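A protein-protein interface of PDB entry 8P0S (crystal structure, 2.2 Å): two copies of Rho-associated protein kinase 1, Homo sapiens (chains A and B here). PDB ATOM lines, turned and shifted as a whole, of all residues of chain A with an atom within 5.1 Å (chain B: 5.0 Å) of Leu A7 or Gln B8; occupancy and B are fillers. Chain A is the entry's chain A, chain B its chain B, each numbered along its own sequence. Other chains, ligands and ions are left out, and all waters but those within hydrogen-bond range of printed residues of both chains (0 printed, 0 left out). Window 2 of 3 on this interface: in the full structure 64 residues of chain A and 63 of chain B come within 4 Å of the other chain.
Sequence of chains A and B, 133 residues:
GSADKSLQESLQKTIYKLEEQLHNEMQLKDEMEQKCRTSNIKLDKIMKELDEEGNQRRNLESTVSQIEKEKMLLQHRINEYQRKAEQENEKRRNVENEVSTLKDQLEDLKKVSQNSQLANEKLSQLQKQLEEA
The side-chain carboxylate (OD1) of Asp A4 lies close to the side-chain carboxylate (OD1) of Asp B4 (2.8 Å). The side-chain amide nitrogen (NE2) of Gln B8 is in hydrogen-bond range of the side-chain carboxylate (OD2) of Asp A4 (2.6 Å).
NE2 of Gln B8 sits close to N of Lys B5 (3.4 Å). The side-chain hydroxyl (OG) of Ser B10 sits at hydrogen-bond distance from the backbone carbonyl oxygen (O) of Leu B7 (3.0 Å). OG of Ser A10 is in hydrogen-bond range of O of Leu A7 (2.6 Å). The side-chain carboxylate of Asp A4 sits at hydrogen-bond distance from the side-chain amide nitrogen of Gln A8 (2.9 Å). The backbone carbonyl oxygen (O) of Asp B4 is in hydrogen-bond range of the side-chain amide nitrogen (NE2) of Gln B8 (2.8 Å).
CD2 of Leu A7 touches OE1 of Gln B8 (3.1 Å). Leu B7 touches Gln A8 (CD1 to OE1, 3.7 Å). CG of Gln B8 touches CG of Gln A8 (3.8 Å). Leu B11 touches Gln A8. Gln B8 touches Leu A11. Leu B11 touches Leu A11. Gln B12 touches Leu A11 (NE2 to CD2, 3.6 Å).
Printed residues of chain B within 4 Å of Asp A4: Asp B4 and Gln B8. Lys A5 touches none of the printed residues of chain B. Leu A7 touches just one residue of chain B: Gln B8. Of the printed residues of chain A, Asp B4 touches Asp A4. Lys B5 touches none of the printed residues of chain A. Printed residues of chain A within 4 Å of Leu B7: Gln A8 (3.7 Å). Gln B8 touches just these residues of chain A: Asp A4, Leu A7, Gln A8 and Leu A11. Of the printed residues of chain A, Leu B11 touches Gln A8 and Leu A11. Printed residues of chain A within 4 Å of Gln B12: Leu A11. The nearest printed residue of chain A that does not touch Asp B4 is Gln A8 (4.1 Å).
Hydrophobic or aromatic side chains of chain A within 4 Å of the printed part of chain B: Leu A7 and Leu A11. Among the printed residues, no Asp or Glu carboxylate lies within 4 Å of a Lys or Arg side-chain nitrogen of the other chain.
Asp A4 touches its own counterpart, Asp B4. Leu A7 touches Gln B8, and with the chains exchanged Gln A8 touches Leu B7. Gln A8 touches its own counterpart, Gln B8. Leu B11 touches its own counterpart, Leu A11. Positions printed for both chains: 4, 5, 6, 7, 8, 9, 10 and 11. Of the 9 pairs that touch across the chains among the printed residues, 7 have their exchanged pair printed and touching as well.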
ATOM      1  N   ALA A   3      12.715 -24.544  -3.757  1.00  0.00           N
ATOM      2  CA  ALA A   3      11.904 -24.394  -4.955  1.00  0.00           C
ATOM      3  C   ALA A   3      10.525 -23.876  -4.596  1.00  0.00           C
ATOM      4  O   ALA A   3       9.971 -23.014  -5.289  1.00  0.00           O
ATOM      5  CB  ALA A   3      11.777 -25.729  -5.686  1.00  0.00           C
ATOM      6  N   ASP A   4       9.952 -24.424  -3.526  1.00  0.00           N
ATOM      7  CA  ASP A   4       8.616 -24.044  -3.087  1.00  0.00           C
ATOM      8  C   ASP A   4       8.592 -22.590  -2.605  1.00  0.00           C
ATOM      9  O   ASP A   4       7.676 -21.828  -2.939  1.00  0.00           O
ATOM     10  CB  ASP A   4       8.174 -25.019  -1.999  1.00  0.00           C
ATOM     11  CG  ASP A   4       7.011 -24.512  -1.204  1.00  0.00           C
ATOM     12  OD1 ASP A   4       7.204 -24.164  -0.012  1.00  0.00           O
ATOM     13  OD2 ASP A   4       5.892 -24.496  -1.758  1.00  0.00           O
ATOM     14  N   LYS A   5       9.618 -22.184  -1.861  1.00  0.00           N
ATOM     15  CA  LYS A   5       9.754 -20.814  -1.394  1.00  0.00           C
ATOM     16  C   LYS A   5      10.062 -19.853  -2.522  1.00  0.00           C
ATOM     17  O   LYS A   5       9.838 -18.650  -2.367  1.00  0.00           O
ATOM     18  CB  LYS A   5      10.854 -20.719  -0.328  1.00  0.00           C
ATOM     19  CG  LYS A   5      10.358 -20.843   1.120  1.00  0.00           C
ATOM     20  CD  LYS A   5       9.874 -22.268   1.467  1.00  0.00           C
ATOM     21  CE  LYS A   5       9.562 -22.432   2.965  1.00  0.00           C
ATOM     22  NZ  LYS A   5      10.745 -22.836   3.778  1.00  0.00           N
ATOM     23  N   SER A   6      10.581 -20.331  -3.646  1.00  0.00           N
ATOM     24  CA  SER A   6      10.749 -19.408  -4.750  1.00  0.00           C
ATOM     25  C   SER A   6       9.480 -19.275  -5.562  1.00  0.00           C
ATOM     26  O   SER A   6       9.203 -18.199  -6.090  1.00  0.00           O
ATOM     27  CB  SER A   6      11.889 -19.844  -5.665  1.00  0.00           C
ATOM     28  OG  SER A   6      12.491 -18.699  -6.250  1.00  0.00           O
ATOM     29  N   LEU A   7       8.713 -20.354  -5.706  1.00  0.00           N
ATOM     30  CA  LEU A   7       7.414 -20.209  -6.332  1.00  0.00           C
ATOM     31  C   LEU A   7       6.548 -19.236  -5.530  1.00  0.00           C
ATOM     32  O   LEU A   7       5.899 -18.352  -6.104  1.00  0.00           O
ATOM     33  CB  LEU A   7       6.757 -21.579  -6.472  1.00  0.00           C
ATOM     34  CG  LEU A   7       5.297 -21.665  -6.897  1.00  0.00           C
ATOM     35  CD1 LEU A   7       5.025 -20.718  -8.053  1.00  0.00           C
ATOM     36  CD2 LEU A   7       4.983 -23.069  -7.326  1.00  0.00           C
ATOM     37  N   GLN A   8       6.572 -19.351  -4.196  1.00  0.00           N
ATOM     38  CA  GLN A   8       5.756 -18.470  -3.365  1.00  0.00           C
ATOM     39  C   GLN A   8       6.206 -17.036  -3.477  1.00  0.00           C
ATOM     40  O   GLN A   8       5.373 -16.120  -3.452  1.00  0.00           O
ATOM     41  CB  GLN A   8       5.799 -18.931  -1.912  1.00  0.00           C
ATOM     42  CG  GLN A   8       5.040 -20.243  -1.723  1.00  0.00           C
ATOM     43  CD  GLN A   8       5.198 -20.790  -0.335  1.00  0.00           C
ATOM     44  OE1 GLN A   8       5.325 -20.032   0.625  1.00  0.00           O
ATOM     45  NE2 GLN A   8       5.213 -22.114  -0.216  1.00  0.00           N
ATOM     46  N   GLU A   9       7.510 -16.819  -3.629  1.00  0.00           N
ATOM     47  CA  GLU A   9       8.022 -15.461  -3.784  1.00  0.00           C
ATOM     48  C   GLU A   9       7.512 -14.847  -5.073  1.00  0.00           C
ATOM     49  O   GLU A   9       7.071 -13.692  -5.097  1.00  0.00           O
ATOM     50  CB  GLU A   9       9.552 -15.460  -3.787  1.00  0.00           C
ATOM     51  CG  GLU A   9      10.215 -14.217  -3.211  1.00  0.00           C
ATOM     52  CD  GLU A   9      10.411 -14.307  -1.702  1.00  0.00           C
ATOM     53  OE1 GLU A   9      10.032 -15.349  -1.114  1.00  0.00           O
ATOM     54  OE2 GLU A   9      10.959 -13.346  -1.104  1.00  0.00           O
ATOM     55  N   SER A  10       7.572 -15.607  -6.162  1.00  0.00           N
ATOM     56  CA  SER A  10       7.071 -15.083  -7.416  1.00  0.00           C
ATOM     57  C   SER A  10       5.566 -14.826  -7.343  1.00  0.00           C
ATOM     58  O   SER A  10       5.081 -13.850  -7.929  1.00  0.00           O
ATOM     59  CB  SER A  10       7.423 -16.042  -8.554  1.00  0.00           C
ATOM     60  OG  SER A  10       6.839 -17.333  -8.355  1.00  0.00           O
ATOM     61  N   LEU A  11       4.807 -15.668  -6.631  1.00  0.00           N
ATOM     62  CA  LEU A  11       3.381 -15.379  -6.512  1.00  0.00           C
ATOM     63  C   LEU A  11       3.128 -14.101  -5.715  1.00  0.00           C
ATOM     64  O   LEU A  11       2.319 -13.267  -6.133  1.00  0.00           O
ATOM     65  CB  LEU A  11       2.655 -16.564  -5.899  1.00  0.00           C
ATOM     66  CG  LEU A  11       2.651 -17.739  -6.886  1.00  0.00           C
ATOM     67  CD1 LEU A  11       2.209 -19.023  -6.206  1.00  0.00           C
ATOM     68  CD2 LEU A  11       1.810 -17.446  -8.113  1.00  0.00           C
ATOM     69  N   ASP B   4       2.588 -27.008   2.200  1.00  0.00           N
ATOM     70  CA  ASP B   4       3.287 -26.358   1.089  1.00  0.00           C
ATOM     71  C   ASP B   4       2.332 -26.002  -0.051  1.00  0.00           C
ATOM     72  O   ASP B   4       2.210 -24.830  -0.441  1.00  0.00           O
ATOM     73  CB  ASP B   4       4.387 -27.298   0.578  1.00  0.00           C
ATOM     74  CG  ASP B   4       5.788 -26.794   0.871  1.00  0.00           C
ATOM     75  OD1 ASP B   4       5.940 -25.937   1.774  1.00  0.00           O
ATOM     76  OD2 ASP B   4       6.739 -27.267   0.198  1.00  0.00           O
ATOM     77  N   LYS B   5       1.680 -27.024  -0.634  1.00  0.00           N
ATOM     78  CA  LYS B   5       0.746 -26.814  -1.740  1.00  0.00           C
ATOM     79  C   LYS B   5      -0.413 -25.915  -1.328  1.00  0.00           C
ATOM     80  O   LYS B   5      -0.881 -25.094  -2.126  1.00  0.00           O
ATOM     81  CB  LYS B   5       0.198 -28.156  -2.248  1.00  0.00           C
ATOM     82  CG  LYS B   5       1.141 -29.349  -2.136  1.00  0.00           C
ATOM     83  CD  LYS B   5       0.668 -30.497  -3.030  1.00  0.00           C
ATOM     84  CE  LYS B   5       0.064 -31.623  -2.186  1.00  0.00           C
ATOM     85  NZ  LYS B   5      -0.909 -32.473  -2.936  1.00  0.00           N
ATOM     86  N   SER B   6      -0.924 -26.099  -0.104  1.00  0.00           N
ATOM     87  CA  SER B   6      -1.907 -25.170   0.437  1.00  0.00           C
ATOM     88  C   SER B   6      -1.463 -23.735   0.205  1.00  0.00           C
ATOM     89  O   SER B   6      -2.232 -22.915  -0.309  1.00  0.00           O
ATOM     90  CB  SER B   6      -2.127 -25.422   1.933  1.00  0.00           C
ATOM     91  OG  SER B   6      -3.048 -26.465   2.156  1.00  0.00           O
ATOM     92  N   LEU B   7      -0.197 -23.433   0.522  1.00  0.00           N
ATOM     93  CA  LEU B   7       0.259 -22.050   0.490  1.00  0.00           C
ATOM     94  C   LEU B   7       0.289 -21.521  -0.934  1.00  0.00           C
ATOM     95  O   LEU B   7      -0.212 -20.423  -1.206  1.00  0.00           O
ATOM     96  CB  LEU B   7       1.633 -21.915   1.146  1.00  0.00           C
ATOM     97  CG  LEU B   7       1.679 -21.889   2.680  1.00  0.00           C
ATOM     98  CD1 LEU B   7       3.099 -21.646   3.132  1.00  0.00           C
ATOM     99  CD2 LEU B   7       0.768 -20.835   3.253  1.00  0.00           C
ATOM    100  N   GLN B   8       0.849 -22.297  -1.865  1.00  0.00           N
ATOM    101  CA  GLN B   8       0.885 -21.854  -3.251  1.00  0.00           C
ATOM    102  C   GLN B   8      -0.508 -21.754  -3.856  1.00  0.00           C
ATOM    103  O   GLN B   8      -0.719 -20.965  -4.786  1.00  0.00           O
ATOM    104  CB  GLN B   8       1.731 -22.802  -4.089  1.00  0.00           C
ATOM    105  CG  GLN B   8       3.114 -23.015  -3.556  1.00  0.00           C
ATOM    106  CD  GLN B   8       3.589 -24.404  -3.856  1.00  0.00           C
ATOM    107  OE1 GLN B   8       3.906 -24.727  -4.999  1.00  0.00           O
ATOM    108  NE2 GLN B   8       3.611 -25.253  -2.838  1.00  0.00           N
ATOM    109  N   GLU B   9      -1.456 -22.558  -3.369  1.00  0.00           N
ATOM    110  CA  GLU B   9      -2.809 -22.501  -3.897  1.00  0.00           C
ATOM    111  C   GLU B   9      -3.555 -21.296  -3.344  1.00  0.00           C
ATOM    112  O   GLU B   9      -4.246 -20.620  -4.102  1.00  0.00           O
ATOM    113  CB  GLU B   9      -3.573 -23.815  -3.620  1.00  0.00           C
ATOM    114  CG  GLU B   9      -4.288 -23.934  -2.256  1.00  0.00           C
ATOM    115  CD  GLU B   9      -5.287 -25.100  -2.175  1.00  0.00           C
ATOM    116  OE1 GLU B   9      -6.345 -25.012  -2.844  1.00  0.00           O
ATOM    117  OE2 GLU B   9      -5.021 -26.087  -1.435  1.00  0.00           O
ATOM    118  N   SER B  10      -3.413 -20.980  -2.045  1.00  0.00           N
ATOM    119  CA  SER B  10      -4.049 -19.752  -1.548  1.00  0.00           C
ATOM    120  C   SER B  10      -3.438 -18.513  -2.193  1.00  0.00           C
ATOM    121  O   SER B  10      -4.129 -17.505  -2.402  1.00  0.00           O
ATOM    122  CB  SER B  10      -3.947 -19.649  -0.017  1.00  0.00           C
ATOM    123  OG  SER B  10      -2.693 -20.111   0.488  1.00  0.00           O
ATOM    124  N   LEU B  11      -2.153 -18.562  -2.532  1.00  0.00           N
ATOM    125  CA  LEU B  11      -1.544 -17.420  -3.204  1.00  0.00           C
ATOM    126  C   LEU B  11      -2.117 -17.249  -4.599  1.00  0.00           C
ATOM    127  O   LEU B  11      -2.424 -16.129  -5.029  1.00  0.00           O
ATOM    128  CB  LEU B  11      -0.032 -17.608  -3.278  1.00  0.00           C
ATOM    129  CG  LEU B  11       0.697 -17.362  -1.972  1.00  0.00           C
ATOM    130  CD1 LEU B  11       2.141 -17.830  -2.063  1.00  0.00           C
ATOM    131  CD2 LEU B  11       0.628 -15.871  -1.660  1.00  0.00           C
ATOM    132  N   GLN B  12      -2.258 -18.356  -5.323  1.00  0.00           N
ATOM    133  CA  GLN B  12      -2.677 -18.266  -6.713  1.00  0.00           C
ATOM    134  C   GLN B  12      -4.146 -17.896  -6.814  1.00  0.00           C
ATOM    135  O   GLN B  12      -4.547 -17.218  -7.766  1.00  0.00           O
ATOM    136  CB  GLN B  12      -2.364 -19.592  -7.432  1.00  0.00           C
ATOM    137  CG  GLN B  12      -2.713 -19.674  -8.935  1.00  0.00           C
ATOM    138  CD  GLN B  12      -2.282 -18.456  -9.779  1.00  0.00           C
ATOM    139  OE1 GLN B  12      -3.111 -17.596 -10.135  1.00  0.00           O
ATOM    140  NE2 GLN B  12      -0.996 -18.388 -10.109  1.00  0.00           N
